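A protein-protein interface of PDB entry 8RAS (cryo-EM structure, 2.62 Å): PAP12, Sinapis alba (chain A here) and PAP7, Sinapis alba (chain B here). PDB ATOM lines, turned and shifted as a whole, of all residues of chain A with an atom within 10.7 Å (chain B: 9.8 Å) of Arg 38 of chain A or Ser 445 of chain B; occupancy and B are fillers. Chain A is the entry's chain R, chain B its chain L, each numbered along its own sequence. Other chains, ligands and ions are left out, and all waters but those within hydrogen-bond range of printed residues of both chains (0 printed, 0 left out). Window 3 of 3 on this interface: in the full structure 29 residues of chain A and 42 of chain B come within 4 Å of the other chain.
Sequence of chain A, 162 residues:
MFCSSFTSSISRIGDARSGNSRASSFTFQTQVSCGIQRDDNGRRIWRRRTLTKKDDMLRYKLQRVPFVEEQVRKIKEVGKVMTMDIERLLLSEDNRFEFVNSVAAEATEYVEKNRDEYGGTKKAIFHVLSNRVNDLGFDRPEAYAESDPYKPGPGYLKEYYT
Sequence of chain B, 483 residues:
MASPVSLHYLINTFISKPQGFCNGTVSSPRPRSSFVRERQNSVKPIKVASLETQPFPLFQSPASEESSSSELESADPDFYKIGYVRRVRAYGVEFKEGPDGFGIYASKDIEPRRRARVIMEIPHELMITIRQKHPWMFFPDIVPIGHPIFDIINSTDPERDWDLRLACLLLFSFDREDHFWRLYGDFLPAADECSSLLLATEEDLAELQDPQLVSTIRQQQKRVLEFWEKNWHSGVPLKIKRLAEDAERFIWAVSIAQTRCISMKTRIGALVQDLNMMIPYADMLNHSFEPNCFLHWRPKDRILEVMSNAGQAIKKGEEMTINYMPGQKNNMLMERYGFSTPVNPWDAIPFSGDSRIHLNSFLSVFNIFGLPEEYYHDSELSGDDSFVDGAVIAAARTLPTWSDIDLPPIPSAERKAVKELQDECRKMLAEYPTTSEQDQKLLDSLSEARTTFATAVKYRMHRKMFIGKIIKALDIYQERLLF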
ATOM      1  N   GLY A  35       0.410 -32.770 -22.145  1.00  0.00           N
ATOM      2  CA  GLY A  35       1.216 -31.824 -21.397  1.00  0.00           C
ATOM      3  C   GLY A  35       0.967 -30.382 -21.792  1.00  0.00           C
ATOM      4  O   GLY A  35       1.470 -29.458 -21.152  1.00  0.00           O
ATOM      5  N   ILE A  36       0.188 -30.189 -22.851  1.00  0.00           N
ATOM      6  CA  ILE A  36      -0.134 -28.858 -23.351  1.00  0.00           C
ATOM      7  C   ILE A  36      -1.365 -28.340 -22.624  1.00  0.00           C
ATOM      8  O   ILE A  36      -2.395 -29.024 -22.558  1.00  0.00           O
ATOM      9  CB  ILE A  36      -0.360 -28.880 -24.871  1.00  0.00           C
ATOM     10  CG1 ILE A  36       0.947 -29.193 -25.598  1.00  0.00           C
ATOM     11  CG2 ILE A  36      -0.929 -27.554 -25.345  1.00  0.00           C
ATOM     12  CD1 ILE A  36       0.837 -29.115 -27.101  1.00  0.00           C
ATOM     13  N   GLN A  37      -1.262 -27.133 -22.073  1.00  0.00           N
ATOM     14  CA  GLN A  37      -2.377 -26.500 -21.388  1.00  0.00           C
ATOM     15  C   GLN A  37      -2.247 -24.991 -21.527  1.00  0.00           C
ATOM     16  O   GLN A  37      -1.156 -24.439 -21.359  1.00  0.00           O
ATOM     17  CB  GLN A  37      -2.429 -26.899 -19.909  1.00  0.00           C
ATOM     18  CG  GLN A  37      -3.612 -26.318 -19.152  1.00  0.00           C
ATOM     19  CD  GLN A  37      -4.940 -26.656 -19.800  1.00  0.00           C
ATOM     20  OE1 GLN A  37      -5.543 -25.824 -20.478  1.00  0.00           O
ATOM     21  NE2 GLN A  37      -5.403 -27.883 -19.593  1.00  0.00           N
ATOM     22  N   ARG A  38      -3.361 -24.334 -21.833  1.00  0.00           N
ATOM     23  CA  ARG A  38      -3.372 -22.886 -21.997  1.00  0.00           C
ATOM     24  C   ARG A  38      -4.503 -22.247 -21.199  1.00  0.00           C
ATOM     25  O   ARG A  38      -5.442 -22.924 -20.781  1.00  0.00           O
ATOM     26  CB  ARG A  38      -3.498 -22.516 -23.476  1.00  0.00           C
ATOM     27  CG  ARG A  38      -2.178 -22.513 -24.221  1.00  0.00           C
ATOM     28  CD  ARG A  38      -2.281 -21.761 -25.538  1.00  0.00           C
ATOM     29  NE  ARG A  38      -2.774 -22.612 -26.614  1.00  0.00           N
ATOM     30  CZ  ARG A  38      -2.000 -23.224 -27.500  1.00  0.00           C
ATOM     31  NH1 ARG A  38      -0.684 -23.099 -27.472  1.00  0.00           N
ATOM     32  NH2 ARG A  38      -2.562 -23.984 -28.436  1.00  0.00           N
ATOM     33  N   ARG A  44       0.634 -20.037 -22.633  1.00  0.00           N
ATOM     34  CA  ARG A  44       0.893 -21.435 -22.313  1.00  0.00           C
ATOM     35  C   ARG A  44       1.403 -21.591 -20.885  1.00  0.00           C
ATOM     36  O   ARG A  44       2.182 -20.771 -20.401  1.00  0.00           O
ATOM     37  CB  ARG A  44       1.905 -22.033 -23.292  1.00  0.00           C
ATOM     38  CG  ARG A  44       1.366 -22.255 -24.693  1.00  0.00           C
ATOM     39  CD  ARG A  44       2.457 -22.754 -25.623  1.00  0.00           C
ATOM     40  NE  ARG A  44       3.069 -23.979 -25.128  1.00  0.00           N
ATOM     41  CZ  ARG A  44       2.756 -25.197 -25.547  1.00  0.00           C
ATOM     42  NH1 ARG A  44       1.837 -25.392 -26.479  1.00  0.00           N
ATOM     43  NH2 ARG A  44       3.381 -26.246 -25.019  1.00  0.00           N
ATOM     44  N   ILE A  45       0.957 -22.650 -20.214  1.00  0.00           N
ATOM     45  CA  ILE A  45       1.413 -22.987 -18.873  1.00  0.00           C
ATOM     46  C   ILE A  45       2.102 -24.343 -18.929  1.00  0.00           C
ATOM     47  O   ILE A  45       1.660 -25.250 -19.644  1.00  0.00           O
ATOM     48  CB  ILE A  45       0.260 -22.987 -17.847  1.00  0.00           C
ATOM     49  CG1 ILE A  45      -0.706 -24.147 -18.095  1.00  0.00           C
ATOM     50  CG2 ILE A  45      -0.483 -21.663 -17.883  1.00  0.00           C
ATOM     51  CD1 ILE A  45      -1.238 -24.776 -16.827  1.00  0.00           C
ATOM     52  N   TRP A  46       3.208 -24.467 -18.199  1.00  0.00           N
ATOM     53  CA  TRP A  46       3.986 -25.696 -18.198  1.00  0.00           C
ATOM     54  C   TRP A  46       4.642 -25.865 -16.837  1.00  0.00           C
ATOM     55  O   TRP A  46       4.835 -24.899 -16.093  1.00  0.00           O
ATOM     56  CB  TRP A  46       5.038 -25.698 -19.315  1.00  0.00           C
ATOM     57  CG  TRP A  46       5.771 -24.399 -19.454  1.00  0.00           C
ATOM     58  CD1 TRP A  46       5.334 -23.275 -20.094  1.00  0.00           C
ATOM     59  CD2 TRP A  46       7.071 -24.089 -18.943  1.00  0.00           C
ATOM     60  NE1 TRP A  46       6.281 -22.285 -20.011  1.00  0.00           N
ATOM     61  CE2 TRP A  46       7.358 -22.760 -19.310  1.00  0.00           C
ATOM     62  CE3 TRP A  46       8.022 -24.805 -18.210  1.00  0.00           C
ATOM     63  CZ2 TRP A  46       8.553 -22.133 -18.970  1.00  0.00           C
ATOM     64  CZ3 TRP A  46       9.207 -24.181 -17.873  1.00  0.00           C
ATOM     65  CH2 TRP A  46       9.463 -22.858 -18.253  1.00  0.00           C
ATOM     66  N   ARG A  47       4.982 -27.110 -16.519  1.00  0.00           N
ATOM     67  CA  ARG A  47       5.572 -27.448 -15.233  1.00  0.00           C
ATOM     68  C   ARG A  47       7.079 -27.243 -15.283  1.00  0.00           C
ATOM     69  O   ARG A  47       7.759 -27.799 -16.151  1.00  0.00           O
ATOM     70  CB  ARG A  47       5.247 -28.893 -14.854  1.00  0.00           C
ATOM     71  CG  ARG A  47       5.817 -29.320 -13.513  1.00  0.00           C
ATOM     72  CD  ARG A  47       5.570 -30.795 -13.252  1.00  0.00           C
ATOM     73  NE  ARG A  47       6.278 -31.645 -14.201  1.00  0.00           N
ATOM     74  CZ  ARG A  47       7.559 -31.974 -14.101  1.00  0.00           C
ATOM     75  NH1 ARG A  47       8.309 -31.538 -13.102  1.00  0.00           N
ATOM     76  NH2 ARG A  47       8.101 -32.760 -15.026  1.00  0.00           N
ATOM     77  N   PRO B  99       8.232 -24.230 -22.864  1.00  0.00           N
ATOM     78  CA  PRO B  99       7.080 -25.144 -22.915  1.00  0.00           C
ATOM     79  C   PRO B  99       7.376 -26.443 -23.641  1.00  0.00           C
ATOM     80  O   PRO B  99       6.832 -27.490 -23.267  1.00  0.00           O
ATOM     81  CB  PRO B  99       6.009 -24.318 -23.642  1.00  0.00           C
ATOM     82  CG  PRO B  99       6.770 -23.281 -24.398  1.00  0.00           C
ATOM     83  CD  PRO B  99       7.968 -22.960 -23.558  1.00  0.00           C
ATOM     84  N   GLU B 437      -2.214 -25.349 -43.019  1.00  0.00           N
ATOM     85  CA  GLU B 437      -2.597 -24.124 -42.322  1.00  0.00           C
ATOM     86  C   GLU B 437      -3.682 -24.399 -41.289  1.00  0.00           C
ATOM     87  O   GLU B 437      -3.648 -23.857 -40.177  1.00  0.00           O
ATOM     88  CB  GLU B 437      -3.060 -23.058 -43.319  1.00  0.00           C
ATOM     89  CG  GLU B 437      -2.165 -22.842 -44.554  1.00  0.00           C
ATOM     90  CD  GLU B 437      -2.219 -23.970 -45.578  1.00  0.00           C
ATOM     91  OE1 GLU B 437      -1.724 -23.764 -46.707  1.00  0.00           O
ATOM     92  OE2 GLU B 437      -2.760 -25.053 -45.269  1.00  0.00           O
ATOM     93  N   GLN B 438      -4.658 -25.242 -41.638  1.00  0.00           N
ATOM     94  CA  GLN B 438      -5.672 -25.624 -40.662  1.00  0.00           C
ATOM     95  C   GLN B 438      -5.065 -26.427 -39.518  1.00  0.00           C
ATOM     96  O   GLN B 438      -5.526 -26.319 -38.378  1.00  0.00           O
ATOM     97  CB  GLN B 438      -6.799 -26.401 -41.349  1.00  0.00           C
ATOM     98  CG  GLN B 438      -6.562 -27.894 -41.504  1.00  0.00           C
ATOM     99  CD  GLN B 438      -7.222 -28.704 -40.406  1.00  0.00           C
ATOM    100  OE1 GLN B 438      -8.430 -28.607 -40.189  1.00  0.00           O
ATOM    101  NE2 GLN B 438      -6.432 -29.508 -39.706  1.00  0.00           N
ATOM    102  N   ASP B 439      -4.024 -27.219 -39.794  1.00  0.00           N
ATOM    103  CA  ASP B 439      -3.330 -27.927 -38.723  1.00  0.00           C
ATOM    104  C   ASP B 439      -2.637 -26.954 -37.779  1.00  0.00           C
ATOM    105  O   ASP B 439      -2.672 -27.132 -36.554  1.00  0.00           O
ATOM    106  CB  ASP B 439      -2.325 -28.915 -39.312  1.00  0.00           C
ATOM    107  CG  ASP B 439      -2.968 -30.224 -39.723  1.00  0.00           C
ATOM    108  OD1 ASP B 439      -3.982 -30.611 -39.104  1.00  0.00           O
ATOM    109  OD2 ASP B 439      -2.458 -30.869 -40.663  1.00  0.00           O
ATOM    110  N   GLN B 440      -1.998 -25.919 -38.329  1.00  0.00           N
ATOM    111  CA  GLN B 440      -1.375 -24.903 -37.486  1.00  0.00           C
ATOM    112  C   GLN B 440      -2.417 -24.165 -36.655  1.00  0.00           C
ATOM    113  O   GLN B 440      -2.186 -23.862 -35.478  1.00  0.00           O
ATOM    114  CB  GLN B 440      -0.578 -23.923 -38.346  1.00  0.00           C
ATOM    115  CG  GLN B 440       0.079 -22.804 -37.557  1.00  0.00           C
ATOM    116  CD  GLN B 440       0.983 -23.321 -36.455  1.00  0.00           C
ATOM    117  OE1 GLN B 440       2.042 -23.887 -36.719  1.00  0.00           O
ATOM    118  NE2 GLN B 440       0.563 -23.131 -35.209  1.00  0.00           N
ATOM    119  N   LYS B 441      -3.571 -23.861 -37.254  1.00  0.00           N
ATOM    120  CA  LYS B 441      -4.645 -23.220 -36.501  1.00  0.00           C
ATOM    121  C   LYS B 441      -5.151 -24.121 -35.381  1.00  0.00           C
ATOM    122  O   LYS B 441      -5.431 -23.651 -34.271  1.00  0.00           O
ATOM    123  CB  LYS B 441      -5.786 -22.833 -37.441  1.00  0.00           C
ATOM    124  CG  LYS B 441      -5.493 -21.608 -38.288  1.00  0.00           C
ATOM    125  CD  LYS B 441      -5.223 -20.395 -37.414  1.00  0.00           C
ATOM    126  CE  LYS B 441      -4.863 -19.176 -38.247  1.00  0.00           C
ATOM    127  NZ  LYS B 441      -4.659 -17.970 -37.399  1.00  0.00           N
ATOM    128  N   LEU B 442      -5.279 -25.422 -35.655  1.00  0.00           N
ATOM    129  CA  LEU B 442      -5.693 -26.366 -34.621  1.00  0.00           C
ATOM    130  C   LEU B 442      -4.672 -26.423 -33.492  1.00  0.00           C
ATOM    131  O   LEU B 442      -5.040 -26.505 -32.314  1.00  0.00           O
ATOM    132  CB  LEU B 442      -5.898 -27.751 -35.233  1.00  0.00           C
ATOM    133  CG  LEU B 442      -6.134 -28.916 -34.272  1.00  0.00           C
ATOM    134  CD1 LEU B 442      -7.401 -28.696 -33.460  1.00  0.00           C
ATOM    135  CD2 LEU B 442      -6.204 -30.230 -35.033  1.00  0.00           C
ATOM    136  N   LEU B 443      -3.383 -26.390 -33.835  1.00  0.00           N
ATOM    137  CA  LEU B 443      -2.345 -26.350 -32.810  1.00  0.00           C
ATOM    138  C   LEU B 443      -2.450 -25.085 -31.968  1.00  0.00           C
ATOM    139  O   LEU B 443      -2.331 -25.136 -30.738  1.00  0.00           O
ATOM    140  CB  LEU B 443      -0.963 -26.442 -33.454  1.00  0.00           C
ATOM    141  CG  LEU B 443      -0.432 -27.840 -33.758  1.00  0.00           C
ATOM    142  CD1 LEU B 443       0.917 -27.749 -34.443  1.00  0.00           C
ATOM    143  CD2 LEU B 443      -0.337 -28.663 -32.488  1.00  0.00           C
ATOM    144  N   ASP B 444      -2.669 -23.939 -32.615  1.00  0.00           N
ATOM    145  CA  ASP B 444      -2.786 -22.684 -31.880  1.00  0.00           C
ATOM    146  C   ASP B 444      -4.026 -22.661 -30.997  1.00  0.00           C
ATOM    147  O   ASP B 444      -4.023 -22.014 -29.943  1.00  0.00           O
ATOM    148  CB  ASP B 444      -2.802 -21.505 -32.852  1.00  0.00           C
ATOM    149  CG  ASP B 444      -1.425 -20.907 -33.063  1.00  0.00           C
ATOM    150  OD1 ASP B 444      -0.961 -20.151 -32.184  1.00  0.00           O
ATOM    151  OD2 ASP B 444      -0.804 -21.194 -34.108  1.00  0.00           O
ATOM    152  N   SER B 445      -5.089 -23.351 -31.401  1.00  0.00           N
ATOM    153  CA  SER B 445      -6.306 -23.441 -30.607  1.00  0.00           C
ATOM    154  C   SER B 445      -6.290 -24.610 -29.630  1.00  0.00           C
ATOM    155  O   SER B 445      -7.264 -24.798 -28.894  1.00  0.00           O
ATOM    156  CB  SER B 445      -7.527 -23.559 -31.525  1.00  0.00           C
ATOM    157  OG  SER B 445      -7.484 -24.760 -32.275  1.00  0.00           O
ATOM    158  N   LEU B 446      -5.215 -25.392 -29.607  1.00  0.00           N
ATOM    159  CA  LEU B 446      -5.150 -26.585 -28.773  1.00  0.00           C
ATOM    160  C   LEU B 446      -4.892 -26.203 -27.321  1.00  0.00           C
ATOM    161  O   LEU B 446      -4.000 -25.400 -27.030  1.00  0.00           O
ATOM    162  CB  LEU B 446      -4.052 -27.516 -29.281  1.00  0.00           C
ATOM    163  CG  LEU B 446      -4.281 -29.019 -29.136  1.00  0.00           C
ATOM    164  CD1 LEU B 446      -5.765 -29.355 -29.181  1.00  0.00           C
ATOM    165  CD2 LEU B 446      -3.525 -29.775 -30.217  1.00  0.00           C
ATOM    166  N   SER B 447      -5.676 -26.778 -26.406  1.00  0.00           N
ATOM    167  CA  SER B 447      -5.511 -26.481 -24.988  1.00  0.00           C
ATOM    168  C   SER B 447      -5.578 -27.691 -24.068  1.00  0.00           C
ATOM    169  O   SER B 447      -5.194 -27.561 -22.902  1.00  0.00           O
ATOM    170  CB  SER B 447      -6.566 -25.461 -24.534  1.00  0.00           C
ATOM    171  OG  SER B 447      -6.416 -24.234 -25.226  1.00  0.00           O
ATOM    172  N   GLU B 448      -6.048 -28.849 -24.527  1.00  0.00           N
ATOM    173  CA  GLU B 448      -6.194 -30.020 -23.668  1.00  0.00           C
ATOM    174  C   GLU B 448      -5.736 -31.279 -24.392  1.00  0.00           C
ATOM    175  O   GLU B 448      -6.407 -32.316 -24.360  1.00  0.00           O
ATOM    176  CB  GLU B 448      -7.636 -30.170 -23.183  1.00  0.00           C
ATOM    177  CG  GLU B 448      -7.785 -30.942 -21.878  1.00  0.00           C
ATOM    178  CD  GLU B 448      -7.299 -30.159 -20.676  1.00  0.00           C
ATOM    179  OE1 GLU B 448      -7.414 -28.915 -20.688  1.00  0.00           O
ATOM    180  OE2 GLU B 448      -6.804 -30.786 -19.715  1.00  0.00           O
ATOM    181  N   ALA B 449      -4.589 -31.209 -25.061  1.00  0.00           N
ATOM    182  CA  ALA B 449      -4.050 -32.343 -25.793  1.00  0.00           C
ATOM    183  C   ALA B 449      -2.682 -32.731 -25.249  1.00  0.00           C
ATOM    184  O   ALA B 449      -1.924 -31.888 -24.759  1.00  0.00           O
ATOM    185  CB  ALA B 449      -3.943 -32.040 -27.289  1.00  0.00           C
ATOM    186  N   PHE B 453      -0.110 -35.944 -29.230  1.00  0.00           N
ATOM    187  CA  PHE B 453      -1.115 -35.389 -30.132  1.00  0.00           C
ATOM    188  C   PHE B 453      -0.524 -34.272 -30.984  1.00  0.00           C
ATOM    189  O   PHE B 453      -0.606 -34.295 -32.222  1.00  0.00           O
ATOM    190  CB  PHE B 453      -2.297 -34.879 -29.306  1.00  0.00           C
ATOM    191  CG  PHE B 453      -3.531 -34.586 -30.105  1.00  0.00           C
ATOM    192  CD1 PHE B 453      -3.701 -33.356 -30.718  1.00  0.00           C
ATOM    193  CD2 PHE B 453      -4.536 -35.531 -30.221  1.00  0.00           C
ATOM    194  CE1 PHE B 453      -4.841 -33.081 -31.443  1.00  0.00           C
ATOM    195  CE2 PHE B 453      -5.678 -35.263 -30.946  1.00  0.00           C
ATOM    196  CZ  PHE B 453      -5.831 -34.034 -31.556  1.00  0.00           C
ATOM    197  N   ALA B 454       0.102 -33.290 -30.331  1.00  0.00           N
ATOM    198  CA  ALA B 454       0.741 -32.203 -31.058  1.00  0.00           C
ATOM    199  C   ALA B 454       1.899 -32.706 -31.904  1.00  0.00           C
ATOM    200  O   ALA B 454       2.158 -32.163 -32.980  1.00  0.00           O
ATOM    201  CB  ALA B 454       1.221 -31.129 -30.085  1.00  0.00           C
ATOM    202  N   VAL B 457       0.344 -34.111 -35.059  1.00  0.00           N
ATOM    203  CA  VAL B 457      -0.149 -33.005 -35.874  1.00  0.00           C
ATOM    204  C   VAL B 457       1.013 -32.304 -36.568  1.00  0.00           C
ATOM    205  O   VAL B 457       0.947 -31.993 -37.765  1.00  0.00           O
ATOM    206  CB  VAL B 457      -0.969 -32.026 -35.013  1.00  0.00           C
ATOM    207  CG1 VAL B 457      -1.231 -30.742 -35.777  1.00  0.00           C
ATOM    208  CG2 VAL B 457      -2.275 -32.669 -34.585  1.00  0.00           C
ATOM    209  N   LYS B 458       2.099 -32.060 -35.831  1.00  0.00           N
ATOM    210  CA  LYS B 458       3.268 -31.412 -36.409  1.00  0.00           C
ATOM    211  C   LYS B 458       3.912 -32.281 -37.479  1.00  0.00           C
ATOM    212  O   LYS B 458       4.396 -31.765 -38.487  1.00  0.00           O
ATOM    213  CB  LYS B 458       4.276 -31.074 -35.312  1.00  0.00           C
ATOM    214  CG  LYS B 458       3.893 -29.862 -34.483  1.00  0.00           C
ATOM    215  CD  LYS B 458       5.060 -29.365 -33.650  1.00  0.00           C
ATOM    216  CE  LYS B 458       5.276 -30.236 -32.426  1.00  0.00           C
ATOM    217  NZ  LYS B 458       4.230 -30.007 -31.393  1.00  0.00           N
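The backbone carbonyl oxygen (O) of Leu 446 of chain B lies within hydrogen-bond range of the guanidinium group (NH2) of Arg 38 of chain A (2.5 Å). O of Leu 443 of chain B sits at hydrogen-bond distance from NH2 of Arg 38 of chain A, 2.6 Å away. NH2 of Arg 38 of chain A lies within hydrogen-bond range of O of Asp 444 of chain B (2.9 Å). The side-chain carboxylate of Glu 448 of chain B lies within hydrogen-bond range of the side-chain amide nitrogen of Gln 37 of chain A (2.5 Å). The backbone carbonyl oxygen (O) of Ser 447 of chain B sits close to the side-chain amide oxygen (OE1) of Gln 37 of chain A. O of Ser 447 of chain B lies close to O of Ile 36 of chain A (3.2 Å). O of Ala 449 of chain B is in hydrogen-bond range of N of Ile 36 of chain A (3.3 Å).
OG of Ser 445 of chain B lies within hydrogen-bond range of O of Lys 441 of chain B (3.1 Å). The backbone carbonyl oxygen of Leu 442 of chain B is in hydrogen-bond range of the side-chain hydroxyl of Ser 445 of chain B. The side-chain amide nitrogen of Gln 440 of chain B is in hydrogen-bond range of the side-chain carboxylate of Asp 444 of chain B. The backbone carbonyl oxygen of Gln 37 of chain A sits at hydrogen-bond distance from the backbone NH of Ile 45 of chain A (3.0 Å). The side-chain amino group (NZ) of Lys 458 of chain B lies close to the backbone carbonyl oxygen (O) of Ala 454 of chain B, 3.4 Å away.
Among the printed residues, pairs that only touch across the chains: Arg 44 of chain A with Pro 99 of chain B (3.3 Å), Gly 35 of chain A with Ala 449 of chain B (3.6 Å), Ile 36 of chain A with Ala 454 of chain B (3.6 Å), Trp 46 of chain A with Pro 99 of chain B (3.8 Å), Arg 38 of chain A with Ser 447 of chain B (3.8 Å) and Arg 38 of chain A with Ser 445 of chain B (3.9 Å).
Printed residues of chain B within 4 Å of Arg 38 of chain A: Leu 443 (2.6 Å), Asp 444 (2.9 Å), Ser 445 (3.9 Å), Leu 446 (2.5 Å) and Ser 447 (3.8 Å). Ser 445 of chain B touches just one residue of chain A: Arg 38 (3.9 Å). Leu 442 of chain B touches none of the printed residues of chain A. Of chain A, only Arg 38 comes within 4 Å of Leu 446 of chain B. Of the printed residues of chain A, Ser 447 of chain B touches Ile 36 (3.2 Å), Gln 37 (3.0 Å) and Arg 38 (3.8 Å). Of the printed residues of chain B, Arg 44 of chain A touches Pro 99 (3.3 Å). Printed residues of chain A within 4 Å of Leu 443 of chain B: Arg 38 (2.6 Å). Of the printed residues of chain A, Glu 448 of chain B touches Gln 37. Of the printed residues of chain B, Trp 46 of chain A touches Pro 99. Of the printed residues of chain A, Ala 449 of chain B touches Gly 35 (3.6 Å) and Ile 36 (3.3 Å). Val 457 of chain B touches none of the printed residues of chain A. The nearest residue of chain A that does not touch Ser 445 of chain B is Ile 36 of chain A (7.5 Å). The nearest printed residue of chain B that does not touch Arg 44 of chain A is Leu 446 of chain B (5.9 Å).
Hydrophobic or aromatic side chains of chain A that line the printed part of chain B: Ile 36 and Trp 46. Of the 18 printed residues of chain B, 9 touch a printed residue of chain A. Along chain B the printed residues that touch a printed residue of chain A span positions 99 to 454. Among the printed residues, 13 pairs touch across the chains. Among the printed residues, no Asp or Glu carboxylate lies within 4 Å of a Lys or Arg side-chain nitrogen of the other chain.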
